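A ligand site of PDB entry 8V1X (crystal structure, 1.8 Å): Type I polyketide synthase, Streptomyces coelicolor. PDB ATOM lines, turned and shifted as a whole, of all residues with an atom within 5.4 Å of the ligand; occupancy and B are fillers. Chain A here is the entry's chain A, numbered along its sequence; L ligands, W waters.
The backbone NH (N) of Ile 234 lies close to a nitrogen (N7) of the ligand.
N of Ala 48 touches O5 of the ligand, 3.98 Å away.
N of Ala 110 touches N3 of the ligand, at 3.7 Å.
CA of Gly 135 touches O4 of the ligand (3.4 Å).
Arg 137 touches the ligand (N to C6, 3.8 Å).
Val 138 touches the ligand.
Val 173 touches the ligand (CG1 to O11, 3.5 Å).
O of Ser 174 touches C21 of the ligand (3.2 Å).
Thr 175 touches the ligand.
Val 231 touches the ligand.
O of Asp 232 touches C19 of the ligand, 3.1 Å away.
Val 233 touches the ligand.
The nearest printed residue that does not touch the ligand is Gly 53 (4.4 Å).
The backbone carbonyl oxygen (O) of Arg 73 is in hydrogen-bond range of the guanidinium group (NH1) of Arg 83, at 3.3 Å.
The side-chain amide nitrogen (ND2) of Asn 134 sits at hydrogen-bond distance from the backbone carbonyl oxygen (O) of Gly 47.
O of Val 173 is in hydrogen-bond range of NZ of Lys 209, 2.7 Å away.
OD1 of Asp 108 is in hydrogen-bond range of N of Ala 110 (2.7 Å).
O of Ser 174 lies within hydrogen-bond range of N of Val 231 (3.0 Å).
The backbone NH (N) of Val 173 is in hydrogen-bond range of the backbone carbonyl oxygen (O) of His 133 (3.1 Å).
Water W10 lies within hydrogen-bond range of O2 of the ligand and OE1 of Gln 244.
Water W12 lies within hydrogen-bond range of O16 of the ligand (2.6 Å) and N of Arg 73 (2.9 Å).
Water W1 lies within hydrogen-bond range of an oxygen (O1) of the ligand (2.8 Å), the backbone NH (N) of Val 138 (2.8 Å) and the backbone carbonyl oxygen (O) of Ala 136 (3.5 Å).
Water W9 lies within hydrogen-bond range of the backbone carbonyl oxygen of Leu 71 (2.8 Å), the backbone NH of Gly 47 (2.8 Å) and a nitrogen (N5) of the ligand (3.1 Å).
Water W13 bridges OH of Tyr 91 and O2 of the ligand.
Water W3 lies within hydrogen-bond range of the side-chain hydroxyl (OG) of Ser 49 (2.7 Å), the backbone carbonyl oxygen (O) of Leu 71 (3.0 Å), an oxygen (O5) of the ligand (3.3 Å) and the backbone NH (N) of Ala 48 (3.3 Å).
An oxygen (O15) of the ligand lies within salt-bridge range of the guanidinium group of Arg 83, 2.4 Å away.
O13 of the ligand lies within hydrogen-bond range of OH of Tyr 205 (2.5 Å).
The backbone NH of Ser 49 sits close to an oxygen (O5) of the ligand, at 3.4 Å.
An oxygen (O15) of the ligand sits at hydrogen-bond distance from the side-chain hydroxyl (OG) of Ser 49.
The guanidinium group of Arg 73 lies within salt-bridge range of an oxygen (O17) of the ligand (2.8 Å).
N4 of the ligand is in hydrogen-bond range of N of Leu 109 (2.8 Å).
O of Asn 134 is in hydrogen-bond range of O12 of the ligand (2.8 Å).
N of Phe 51 sits at hydrogen-bond distance from O2 of the ligand.
NZ of Lys 209 sits at hydrogen-bond distance from O12 of the ligand, at 2.9 Å.
A nitrogen (N3) of the ligand sits at hydrogen-bond distance from the side-chain carboxylate (OD1) of Asp 108 (2.9 Å).
N of Ala 136 sits at hydrogen-bond distance from O4 of the ligand (3.0 Å).
OG of Ser 150 lies within hydrogen-bond range of N3 of the ligand.
The backbone NH of Gly 50 sits at hydrogen-bond distance from an oxygen (O5) of the ligand, at 3.0 Å.
An oxygen (O8) of the ligand is in hydrogen-bond range of the backbone NH (N) of Leu 52 (3.1 Å).
NE2 of Gln 244 lies within hydrogen-bond range of O14 of the ligand, at 3.1 Å.
O5 of the ligand sits close to O of Gly 47, at 3.1 Å.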
ATOM      1  N   GLY A  47       5.231  19.422 -23.143  1.00  0.00           N
ATOM      2  CA  GLY A  47       4.266  19.022 -22.138  1.00  0.00           C
ATOM      3  C   GLY A  47       3.504  20.188 -21.561  1.00  0.00           C
ATOM      4  O   GLY A  47       2.894  20.031 -20.500  1.00  0.00           O
ATOM      5  N   ALA A  48       3.502  21.344 -22.239  1.00  0.00           N
ATOM      6  CA  ALA A  48       2.785  22.506 -21.700  1.00  0.00           C
ATOM      7  C   ALA A  48       1.277  22.329 -21.687  1.00  0.00           C
ATOM      8  O   ALA A  48       0.578  23.071 -20.972  1.00  0.00           O
ATOM      9  CB  ALA A  48       3.110  23.759 -22.486  1.00  0.00           C
ATOM     10  N   SER A  49       0.750  21.391 -22.466  1.00  0.00           N
ATOM     11  CA  SER A  49      -0.681  21.121 -22.473  1.00  0.00           C
ATOM     12  C   SER A  49      -1.113  20.140 -21.380  1.00  0.00           C
ATOM     13  O   SER A  49      -2.290  19.743 -21.339  1.00  0.00           O
ATOM     14  CB  SER A  49      -1.095  20.595 -23.864  1.00  0.00           C
ATOM     15  OG  SER A  49      -0.453  19.354 -24.086  1.00  0.00           O
ATOM     16  N   GLY A  50      -0.215  19.794 -20.443  1.00  0.00           N
ATOM     17  CA  GLY A  50      -0.503  18.919 -19.342  1.00  0.00           C
ATOM     18  C   GLY A  50      -0.508  19.618 -17.987  1.00  0.00           C
ATOM     19  O   GLY A  50      -0.640  20.833 -17.879  1.00  0.00           O
ATOM     20  N   PHE A  51      -0.430  18.795 -16.934  1.00  0.00           N
ATOM     21  CA  PHE A  51      -0.601  19.229 -15.560  1.00  0.00           C
ATOM     22  C   PHE A  51       0.584  20.062 -15.107  1.00  0.00           C
ATOM     23  O   PHE A  51       0.481  21.276 -14.975  1.00  0.00           O
ATOM     24  CB  PHE A  51      -0.805  18.001 -14.677  1.00  0.00           C
ATOM     25  CG  PHE A  51      -1.022  18.322 -13.212  1.00  0.00           C
ATOM     26  CD1 PHE A  51      -1.555  19.527 -12.828  1.00  0.00           C
ATOM     27  CD2 PHE A  51      -0.714  17.388 -12.242  1.00  0.00           C
ATOM     28  CE1 PHE A  51      -1.752  19.848 -11.491  1.00  0.00           C
ATOM     29  CE2 PHE A  51      -0.878  17.697 -10.895  1.00  0.00           C
ATOM     30  CZ  PHE A  51      -1.397  18.927 -10.520  1.00  0.00           C
ATOM     31  N   LEU A  52       1.733  19.434 -14.886  1.00  0.00           N
ATOM     32  CA  LEU A  52       2.897  20.196 -14.489  1.00  0.00           C
ATOM     33  C   LEU A  52       3.252  21.232 -15.540  1.00  0.00           C
ATOM     34  O   LEU A  52       3.720  22.328 -15.171  1.00  0.00           O
ATOM     35  CB  LEU A  52       4.068  19.264 -14.233  1.00  0.00           C
ATOM     36  CG  LEU A  52       5.392  19.898 -13.866  1.00  0.00           C
ATOM     37  CD1 LEU A  52       5.193  20.808 -12.653  1.00  0.00           C
ATOM     38  CD2 LEU A  52       6.431  18.819 -13.547  1.00  0.00           C
ATOM     39  N   GLY A  53       2.950  20.957 -16.821  1.00  0.00           N
ATOM     40  CA  GLY A  53       3.439  21.831 -17.867  1.00  0.00           C
ATOM     41  C   GLY A  53       2.741  23.161 -17.836  1.00  0.00           C
ATOM     42  O   GLY A  53       3.322  24.185 -18.195  1.00  0.00           O
ATOM     43  N   LEU A  71       5.842  22.894 -27.512  1.00  0.00           N
ATOM     44  CA  LEU A  71       5.568  21.761 -28.392  1.00  0.00           C
ATOM     45  C   LEU A  71       4.242  21.161 -28.016  1.00  0.00           C
ATOM     46  O   LEU A  71       4.099  20.665 -26.895  1.00  0.00           O
ATOM     47  CB  LEU A  71       6.662  20.710 -28.222  1.00  0.00           C
ATOM     48  CG  LEU A  71       6.621  19.570 -29.229  1.00  0.00           C
ATOM     49  CD1 LEU A  71       6.902  20.081 -30.639  1.00  0.00           C
ATOM     50  CD2 LEU A  71       7.608  18.478 -28.823  1.00  0.00           C
ATOM     51  N   VAL A  72       3.280  21.196 -28.937  1.00  0.00           N
ATOM     52  CA  VAL A  72       1.921  20.720 -28.741  1.00  0.00           C
ATOM     53  C   VAL A  72       1.483  19.945 -29.975  1.00  0.00           C
ATOM     54  O   VAL A  72       1.678  20.380 -31.116  1.00  0.00           O
ATOM     55  CB  VAL A  72       0.959  21.892 -28.491  1.00  0.00           C
ATOM     56  CG1 VAL A  72      -0.432  21.356 -28.100  1.00  0.00           C
ATOM     57  CG2 VAL A  72       1.449  22.769 -27.406  1.00  0.00           C
ATOM     58  N   ARG A  73       0.866  18.784 -29.757  1.00  0.00           N
ATOM     59  CA  ARG A  73       0.247  18.021 -30.839  1.00  0.00           C
ATOM     60  C   ARG A  73      -1.068  18.648 -31.284  1.00  0.00           C
ATOM     61  O   ARG A  73      -1.823  19.205 -30.483  1.00  0.00           O
ATOM     62  CB  ARG A  73      -0.025  16.581 -30.401  1.00  0.00           C
ATOM     63  CG  ARG A  73       1.198  15.771 -30.070  1.00  0.00           C
ATOM     64  CD  ARG A  73       0.856  14.374 -29.729  1.00  0.00           C
ATOM     65  NE  ARG A  73       0.200  14.276 -28.428  1.00  0.00           N
ATOM     66  CZ  ARG A  73      -0.187  13.135 -27.849  1.00  0.00           C
ATOM     67  NH1 ARG A  73       0.020  11.953 -28.428  1.00  0.00           N
ATOM     68  NH2 ARG A  73      -0.772  13.184 -26.651  1.00  0.00           N
ATOM     69  N   ARG A  83      -6.093  24.041 -27.376  1.00  0.00           N
ATOM     70  CA  ARG A  83      -5.857  22.970 -26.417  1.00  0.00           C
ATOM     71  C   ARG A  83      -4.972  23.462 -25.262  1.00  0.00           C
ATOM     72  O   ARG A  83      -5.295  23.272 -24.084  1.00  0.00           O
ATOM     73  CB  ARG A  83      -5.195  21.795 -27.134  1.00  0.00           C
ATOM     74  CG  ARG A  83      -6.122  20.867 -27.870  1.00  0.00           C
ATOM     75  CD  ARG A  83      -5.364  19.574 -28.274  1.00  0.00           C
ATOM     76  NE  ARG A  83      -5.142  18.758 -27.098  1.00  0.00           N
ATOM     77  CZ  ARG A  83      -3.968  18.285 -26.721  1.00  0.00           C
ATOM     78  NH1 ARG A  83      -2.895  18.444 -27.472  1.00  0.00           N
ATOM     79  NH2 ARG A  83      -3.865  17.642 -25.562  1.00  0.00           N
ATOM     80  N   TYR A  91      -6.741  24.345 -15.186  1.00  0.00           N
ATOM     81  CA  TYR A  91      -5.881  24.480 -14.013  1.00  0.00           C
ATOM     82  C   TYR A  91      -5.834  25.896 -13.460  1.00  0.00           C
ATOM     83  O   TYR A  91      -5.164  26.130 -12.430  1.00  0.00           O
ATOM     84  CB  TYR A  91      -4.490  24.007 -14.387  1.00  0.00           C
ATOM     85  CG  TYR A  91      -4.414  22.535 -14.572  1.00  0.00           C
ATOM     86  CD1 TYR A  91      -4.586  21.689 -13.501  1.00  0.00           C
ATOM     87  CD2 TYR A  91      -4.186  21.971 -15.815  1.00  0.00           C
ATOM     88  CE1 TYR A  91      -4.538  20.312 -13.655  1.00  0.00           C
ATOM     89  CE2 TYR A  91      -4.110  20.617 -15.972  1.00  0.00           C
ATOM     90  CZ  TYR A  91      -4.305  19.791 -14.893  1.00  0.00           C
ATOM     91  OH  TYR A  91      -4.288  18.429 -15.022  1.00  0.00           O
ATOM     92  N   GLY A 107       3.983  19.865 -33.250  1.00  0.00           N
ATOM     93  CA  GLY A 107       4.861  18.717 -33.391  1.00  0.00           C
ATOM     94  C   GLY A 107       4.445  17.575 -32.483  1.00  0.00           C
ATOM     95  O   GLY A 107       3.355  17.590 -31.910  1.00  0.00           O
ATOM     96  N   ASP A 108       5.307  16.578 -32.364  1.00  0.00           N
ATOM     97  CA  ASP A 108       4.951  15.335 -31.691  1.00  0.00           C
ATOM     98  C   ASP A 108       6.218  14.684 -31.173  1.00  0.00           C
ATOM     99  O   ASP A 108       7.123  14.367 -31.964  1.00  0.00           O
ATOM    100  CB  ASP A 108       4.235  14.379 -32.663  1.00  0.00           C
ATOM    101  CG  ASP A 108       3.595  13.214 -31.976  1.00  0.00           C
ATOM    102  OD1 ASP A 108       4.211  12.662 -31.051  1.00  0.00           O
ATOM    103  OD2 ASP A 108       2.444  12.864 -32.355  1.00  0.00           O
ATOM    104  N   LEU A 109       6.257  14.460 -29.856  1.00  0.00           N
ATOM    105  CA  LEU A 109       7.434  13.841 -29.253  1.00  0.00           C
ATOM    106  C   LEU A 109       7.691  12.466 -29.840  1.00  0.00           C
ATOM    107  O   LEU A 109       8.822  11.974 -29.752  1.00  0.00           O
ATOM    108  CB  LEU A 109       7.244  13.719 -27.741  1.00  0.00           C
ATOM    109  CG  LEU A 109       7.339  14.964 -26.869  1.00  0.00           C
ATOM    110  CD1 LEU A 109       6.898  14.580 -25.489  1.00  0.00           C
ATOM    111  CD2 LEU A 109       8.714  15.486 -26.871  1.00  0.00           C
ATOM    112  N   ALA A 110       6.662  11.823 -30.377  1.00  0.00           N
ATOM    113  CA  ALA A 110       6.772  10.435 -30.850  1.00  0.00           C
ATOM    114  C   ALA A 110       7.178  10.348 -32.313  1.00  0.00           C
ATOM    115  O   ALA A 110       7.207   9.253 -32.873  1.00  0.00           O
ATOM    116  CB  ALA A 110       5.443   9.660 -30.637  1.00  0.00           C
ATOM    117  N   HIS A 133      12.188  19.794 -20.661  1.00  0.00           N
ATOM    118  CA  HIS A 133      11.625  18.599 -21.278  1.00  0.00           C
ATOM    119  C   HIS A 133      10.724  17.877 -20.273  1.00  0.00           C
ATOM    120  O   HIS A 133      11.149  16.993 -19.544  1.00  0.00           O
ATOM    121  CB  HIS A 133      12.718  17.668 -21.801  1.00  0.00           C
ATOM    122  CG  HIS A 133      12.153  16.433 -22.410  1.00  0.00           C
ATOM    123  ND1 HIS A 133      10.860  16.390 -22.909  1.00  0.00           N
ATOM    124  CD2 HIS A 133      12.668  15.194 -22.584  1.00  0.00           C
ATOM    125  CE1 HIS A 133      10.619  15.181 -23.376  1.00  0.00           C
ATOM    126  NE2 HIS A 133      11.683  14.431 -23.164  1.00  0.00           N
ATOM    127  N   ASN A 134       9.484  18.335 -20.214  1.00  0.00           N
ATOM    128  CA  ASN A 134       8.480  17.903 -19.261  1.00  0.00           C
ATOM    129  C   ASN A 134       7.450  16.958 -19.899  1.00  0.00           C
ATOM    130  O   ASN A 134       6.841  16.129 -19.212  1.00  0.00           O
ATOM    131  CB  ASN A 134       7.781  19.157 -18.728  1.00  0.00           C
ATOM    132  CG  ASN A 134       6.437  18.836 -18.096  1.00  0.00           C
ATOM    133  OD1 ASN A 134       6.355  18.404 -16.949  1.00  0.00           O
ATOM    134  ND2 ASN A 134       5.358  19.105 -18.819  1.00  0.00           N
ATOM    135  N   GLY A 135       7.265  17.036 -21.215  1.00  0.00           N
ATOM    136  CA  GLY A 135       6.267  16.209 -21.846  1.00  0.00           C
ATOM    137  C   GLY A 135       6.687  14.741 -21.853  1.00  0.00           C
ATOM    138  O   GLY A 135       7.868  14.398 -22.025  1.00  0.00           O
ATOM    139  N   ALA A 136       5.688  13.899 -21.664  1.00  0.00           N
ATOM    140  CA  ALA A 136       5.834  12.451 -21.707  1.00  0.00           C
ATOM    141  C   ALA A 136       4.444  11.865 -21.710  1.00  0.00           C
ATOM    142  O   ALA A 136       3.492  12.520 -21.308  1.00  0.00           O
ATOM    143  CB  ALA A 136       6.604  11.931 -20.496  1.00  0.00           C
ATOM    144  N   ARG A 137       4.350  10.597 -22.085  1.00  0.00           N
ATOM    145  CA  ARG A 137       3.086   9.858 -22.003  1.00  0.00           C
ATOM    146  C   ARG A 137       3.023   9.110 -20.679  1.00  0.00           C
ATOM    147  O   ARG A 137       3.860   8.239 -20.426  1.00  0.00           O
ATOM    148  CB  ARG A 137       2.933   8.880 -23.167  1.00  0.00           C
ATOM    149  CG  ARG A 137       1.591   8.052 -23.058  1.00  0.00           C
ATOM    150  CD  ARG A 137       0.914   7.959 -24.387  1.00  0.00           C
ATOM    151  NE  ARG A 137      -0.372   7.238 -24.378  1.00  0.00           N
ATOM    152  CZ  ARG A 137      -1.366   7.470 -23.529  1.00  0.00           C
ATOM    153  NH1 ARG A 137      -1.303   8.406 -22.604  1.00  0.00           N
ATOM    154  NH2 ARG A 137      -2.480   6.746 -23.628  1.00  0.00           N
ATOM    155  N   VAL A 138       2.141   9.553 -19.779  1.00  0.00           N
ATOM    156  CA  VAL A 138       2.072   8.994 -18.440  1.00  0.00           C
ATOM    157  C   VAL A 138       0.866   8.069 -18.406  1.00  0.00           C
ATOM    158  O   VAL A 138      -0.267   8.527 -18.265  1.00  0.00           O
ATOM    159  CB  VAL A 138       1.977  10.076 -17.364  1.00  0.00           C
ATOM    160  CG1 VAL A 138       1.891   9.415 -15.986  1.00  0.00           C
ATOM    161  CG2 VAL A 138       3.200  11.003 -17.424  1.00  0.00           C
ATOM    162  N   SER A 150       7.417   8.084 -27.366  1.00  0.00           N
ATOM    163  CA  SER A 150       7.207   9.394 -26.746  1.00  0.00           C
ATOM    164  C   SER A 150       8.226   9.671 -25.649  1.00  0.00           C
ATOM    165  O   SER A 150       8.640  10.821 -25.433  1.00  0.00           O
ATOM    166  CB  SER A 150       5.785   9.487 -26.157  1.00  0.00           C
ATOM    167  OG  SER A 150       4.875   9.624 -27.227  1.00  0.00           O
ATOM    168  N   VAL A 173      12.268  16.345 -16.731  1.00  0.00           N
ATOM    169  CA  VAL A 173      11.410  15.998 -15.604  1.00  0.00           C
ATOM    170  C   VAL A 173      11.352  14.488 -15.563  1.00  0.00           C
ATOM    171  O   VAL A 173      10.923  13.859 -16.527  1.00  0.00           O
ATOM    172  CB  VAL A 173      10.018  16.611 -15.722  1.00  0.00           C
ATOM    173  CG1 VAL A 173       9.198  16.247 -14.503  1.00  0.00           C
ATOM    174  CG2 VAL A 173      10.070  18.126 -15.843  1.00  0.00           C
ATOM    175  N   SER A 174      11.784  13.920 -14.428  1.00  0.00           N
ATOM    176  CA  SER A 174      11.694  12.480 -14.218  1.00  0.00           C
ATOM    177  C   SER A 174      10.903  12.141 -12.966  1.00  0.00           C
ATOM    178  O   SER A 174      10.112  12.969 -12.492  1.00  0.00           O
ATOM    179  CB  SER A 174      13.091  11.897 -14.122  1.00  0.00           C
ATOM    180  OG  SER A 174      13.064  10.528 -14.101  1.00  0.00           O
ATOM    181  N   THR A 175      11.070  10.923 -12.441  1.00  0.00           N
ATOM    182  CA  THR A 175      10.244  10.460 -11.327  1.00  0.00           C
ATOM    183  C   THR A 175      11.085   9.693 -10.317  1.00  0.00           C
ATOM    184  O   THR A 175      11.985   8.945 -10.704  1.00  0.00           O
ATOM    185  CB  THR A 175       9.071   9.545 -11.802  1.00  0.00           C
ATOM    186  OG1 THR A 175       8.471   8.932 -10.660  1.00  0.00           O
ATOM    187  CG2 THR A 175       9.567   8.447 -12.751  1.00  0.00           C
ATOM    188  N   TYR A 205       5.659   2.405 -17.858  1.00  0.00           N
ATOM    189  CA  TYR A 205       5.904   3.839 -17.760  1.00  0.00           C
ATOM    190  C   TYR A 205       7.180   4.123 -16.982  1.00  0.00           C
ATOM    191  O   TYR A 205       8.064   4.875 -17.423  1.00  0.00           O
ATOM    192  CB  TYR A 205       4.724   4.535 -17.092  1.00  0.00           C
ATOM    193  CG  TYR A 205       5.053   5.909 -16.587  1.00  0.00           C
ATOM    194  CD1 TYR A 205       5.380   6.953 -17.466  1.00  0.00           C
ATOM    195  CD2 TYR A 205       5.053   6.186 -15.224  1.00  0.00           C
ATOM    196  CE1 TYR A 205       5.663   8.251 -16.973  1.00  0.00           C
ATOM    197  CE2 TYR A 205       5.334   7.507 -14.736  1.00  0.00           C
ATOM    198  CZ  TYR A 205       5.652   8.478 -15.619  1.00  0.00           C
ATOM    199  OH  TYR A 205       5.912   9.729 -15.164  1.00  0.00           O
ATOM    200  N   LYS A 209      10.864   5.870 -18.223  1.00  0.00           N
ATOM    201  CA  LYS A 209      11.577   6.981 -17.590  1.00  0.00           C
ATOM    202  C   LYS A 209      12.982   6.570 -17.170  1.00  0.00           C
ATOM    203  O   LYS A 209      13.926   7.371 -17.214  1.00  0.00           O
ATOM    204  CB  LYS A 209      10.791   7.513 -16.388  1.00  0.00           C
ATOM    205  CG  LYS A 209       9.375   8.059 -16.745  1.00  0.00           C
ATOM    206  CD  LYS A 209       9.414   9.304 -17.707  1.00  0.00           C
ATOM    207  CE  LYS A 209       9.754  10.554 -16.930  1.00  0.00           C
ATOM    208  NZ  LYS A 209       9.512  11.832 -17.709  1.00  0.00           N
ATOM    209  N   VAL A 231      10.611  13.663  -9.644  1.00  0.00           N
ATOM    210  CA  VAL A 231       9.486  14.187  -8.893  1.00  0.00           C
ATOM    211  C   VAL A 231       8.669  13.041  -8.314  1.00  0.00           C
ATOM    212  O   VAL A 231       8.611  11.953  -8.865  1.00  0.00           O
ATOM    213  CB  VAL A 231       8.623  15.093  -9.788  1.00  0.00           C
ATOM    214  CG1 VAL A 231       7.530  15.709  -9.003  1.00  0.00           C
ATOM    215  CG2 VAL A 231       9.508  16.152 -10.400  1.00  0.00           C
ATOM    216  N   ASP A 232       8.125  13.265  -7.130  1.00  0.00           N
ATOM    217  CA  ASP A 232       7.219  12.294  -6.508  1.00  0.00           C
ATOM    218  C   ASP A 232       5.777  12.610  -6.953  1.00  0.00           C
ATOM    219  O   ASP A 232       5.572  13.316  -7.942  1.00  0.00           O
ATOM    220  CB  ASP A 232       7.353  12.348  -4.988  1.00  0.00           C
ATOM    221  CG  ASP A 232       6.882  11.089  -4.280  1.00  0.00           C
ATOM    222  OD1 ASP A 232       6.840  10.051  -4.910  1.00  0.00           O
ATOM    223  OD2 ASP A 232       6.573  11.184  -3.103  1.00  0.00           O
ATOM    224  N   VAL A 233       4.781  12.203  -6.183  1.00  0.00           N
ATOM    225  CA  VAL A 233       3.389  12.432  -6.555  1.00  0.00           C
ATOM    226  C   VAL A 233       3.042  13.913  -6.419  1.00  0.00           C
ATOM    227  O   VAL A 233       3.354  14.577  -5.417  1.00  0.00           O
ATOM    228  CB  VAL A 233       2.468  11.573  -5.673  1.00  0.00           C
ATOM    229  CG1 VAL A 233       2.854  11.691  -4.202  1.00  0.00           C
ATOM    230  CG2 VAL A 233       1.005  11.994  -5.921  1.00  0.00           C
ATOM    231  N   ILE A 234       2.419  14.468  -7.461  1.00  0.00           N
ATOM    232  CA  ILE A 234       2.117  15.888  -7.521  1.00  0.00           C
ATOM    233  C   ILE A 234       0.663  16.091  -7.140  1.00  0.00           C
ATOM    234  O   ILE A 234      -0.209  15.435  -7.691  1.00  0.00           O
ATOM    235  CB  ILE A 234       2.396  16.450  -8.926  1.00  0.00           C
ATOM    236  CG1 ILE A 234       3.873  16.320  -9.238  1.00  0.00           C
ATOM    237  CG2 ILE A 234       1.994  17.890  -9.035  1.00  0.00           C
ATOM    238  CD1 ILE A 234       4.278  16.556 -10.685  1.00  0.00           C
ATOM    239  N   GLN A 244      -4.633  17.224 -11.343  1.00  0.00           N
ATOM    240  CA  GLN A 244      -5.098  16.218 -12.253  1.00  0.00           C
ATOM    241  C   GLN A 244      -5.968  15.229 -11.496  1.00  0.00           C
ATOM    242  O   GLN A 244      -5.912  15.131 -10.267  1.00  0.00           O
ATOM    243  CB  GLN A 244      -3.912  15.501 -12.904  1.00  0.00           C
ATOM    244  CG  GLN A 244      -3.222  14.533 -11.947  1.00  0.00           C
ATOM    245  CD  GLN A 244      -1.826  14.111 -12.428  1.00  0.00           C
ATOM    246  OE1 GLN A 244      -1.589  13.971 -13.618  1.00  0.00           O
ATOM    247  NE2 GLN A 244      -0.918  13.902 -11.498  1.00  0.00           N
HETATM  248  P1  LIG L   1       0.250  15.042 -18.141  1.00  0.00           P
HETATM  249  O1  LIG L   1      -0.303  13.778 -18.754  1.00  0.00           O
HETATM  250  O2  LIG L   1      -0.721  15.988 -17.455  1.00  0.00           O
HETATM  251  O3  LIG L   1       1.200  15.922 -19.129  1.00  0.00           O
HETATM  252  C1  LIG L   1       1.677  15.078 -20.161  1.00  0.00           C
HETATM  253  C2  LIG L   1       2.197  16.002 -21.245  1.00  0.00           C
HETATM  254  O4  LIG L   1       3.042  15.255 -22.218  1.00  0.00           O
HETATM  255  C3  LIG L   1       0.985  16.666 -21.998  1.00  0.00           C
HETATM  256  O5  LIG L   1       1.315  18.014 -22.327  1.00  0.00           O
HETATM  257  C4  LIG L   1       0.957  15.839 -23.261  1.00  0.00           C
HETATM  258  O6  LIG L   1       0.531  16.463 -24.387  1.00  0.00           O
HETATM  259  C5  LIG L   1       2.615  15.644 -23.377  1.00  0.00           C
HETATM  260  N1  LIG L   1       2.791  14.579 -24.377  1.00  0.00           N
HETATM  261  C6  LIG L   1       2.652  13.187 -24.219  1.00  0.00           C
HETATM  262  N2  LIG L   1       2.936  12.506 -25.339  1.00  0.00           N
HETATM  263  C7  LIG L   1       3.242  13.466 -26.255  1.00  0.00           C
HETATM  264  C8  LIG L   1       3.599  13.394 -27.586  1.00  0.00           C
HETATM  265  N3  LIG L   1       3.724  12.182 -28.223  1.00  0.00           N
HETATM  266  N4  LIG L   1       3.906  14.557 -28.307  1.00  0.00           N
HETATM  267  C9  LIG L   1       3.821  15.725 -27.633  1.00  0.00           C
HETATM  268  N5  LIG L   1       3.474  15.959 -26.358  1.00  0.00           N
HETATM  269  C10 LIG L   1       3.198  14.768 -25.690  1.00  0.00           C
HETATM  270  O7  LIG L   1       1.207  14.297 -17.048  1.00  0.00           O
HETATM  271  P2  LIG L   1       2.117  15.233 -16.031  1.00  0.00           P
HETATM  272  O8  LIG L   1       2.080  16.699 -16.220  1.00  0.00           O
HETATM  273  O9  LIG L   1       2.010  14.591 -14.668  1.00  0.00           O
HETATM  274  O10 LIG L   1       3.695  14.740 -16.535  1.00  0.00           O
HETATM  275  C11 LIG L   1       4.565  15.869 -16.570  1.00  0.00           C
HETATM  276  C12 LIG L   1       5.940  15.308 -16.408  1.00  0.00           C
HETATM  277  O11 LIG L   1       5.896  15.069 -15.042  1.00  0.00           O
HETATM  278  C13 LIG L   1       6.141  13.963 -17.078  1.00  0.00           C
HETATM  279  O12 LIG L   1       7.527  13.935 -17.569  1.00  0.00           O
HETATM  280  C14 LIG L   1       6.022  12.930 -15.943  1.00  0.00           C
HETATM  281  O13 LIG L   1       6.915  11.872 -16.106  1.00  0.00           O
HETATM  282  C15 LIG L   1       6.521  13.791 -14.768  1.00  0.00           C
HETATM  283  N6  LIG L   1       6.044  13.376 -13.448  1.00  0.00           N
HETATM  284  C16 LIG L   1       4.703  13.554 -13.070  1.00  0.00           C
HETATM  285  C17 LIG L   1       4.280  13.167 -11.854  1.00  0.00           C
HETATM  286  C18 LIG L   1       2.873  13.380 -11.529  1.00  0.00           C
HETATM  287  O14 LIG L   1       2.063  13.921 -12.258  1.00  0.00           O
HETATM  288  N7  LIG L   1       2.424  12.919 -10.338  1.00  0.00           N
HETATM  289  C19 LIG L   1       5.196  12.514 -10.875  1.00  0.00           C
HETATM  290  C20 LIG L   1       6.538  12.331 -11.414  1.00  0.00           C
HETATM  291  C21 LIG L   1       6.920  12.751 -12.568  1.00  0.00           C
HETATM  292  P3  LIG L   1      -1.143  16.041 -24.931  1.00  0.00           P
HETATM  293  O15 LIG L   1      -1.902  17.123 -24.220  1.00  0.00           O
HETATM  294  O16 LIG L   1      -0.962  16.181 -26.452  1.00  0.00           O
HETATM  295  O17 LIG L   1      -1.254  14.634 -24.341  1.00  0.00           O
HETATM  296  O   HOH W   1       0.265  11.591 -20.390  1.00  0.00           O
HETATM  297  O   HOH W   2       2.698  18.288 -18.068  1.00  0.00           O
HETATM  298  O   HOH W   3       2.038  19.980 -24.838  1.00  0.00           O
HETATM  299  O   HOH W   4      -1.650  11.877 -17.232  1.00  0.00           O
HETATM  300  O   HOH W   5      -0.413  12.122 -22.850  1.00  0.00           O
HETATM  301  O   HOH W   6       1.886  10.195 -12.464  1.00  0.00           O
HETATM  302  O   HOH W   7       0.397  12.359 -14.658  1.00  0.00           O
HETATM  303  O   HOH W   8       9.499  14.282 -19.791  1.00  0.00           O
HETATM  304  O   HOH W   9       5.285  18.410 -25.806  1.00  0.00           O
HETATM  305  O   HOH W  10      -2.720  14.912 -16.303  1.00  0.00           O
HETATM  306  O   HOH W  11       4.667  10.086 -12.863  1.00  0.00           O
HETATM  307  O   HOH W  12       0.907  17.921 -26.983  1.00  0.00           O
HETATM  308  O   HOH W  13      -3.825  16.864 -17.172  1.00  0.00           O
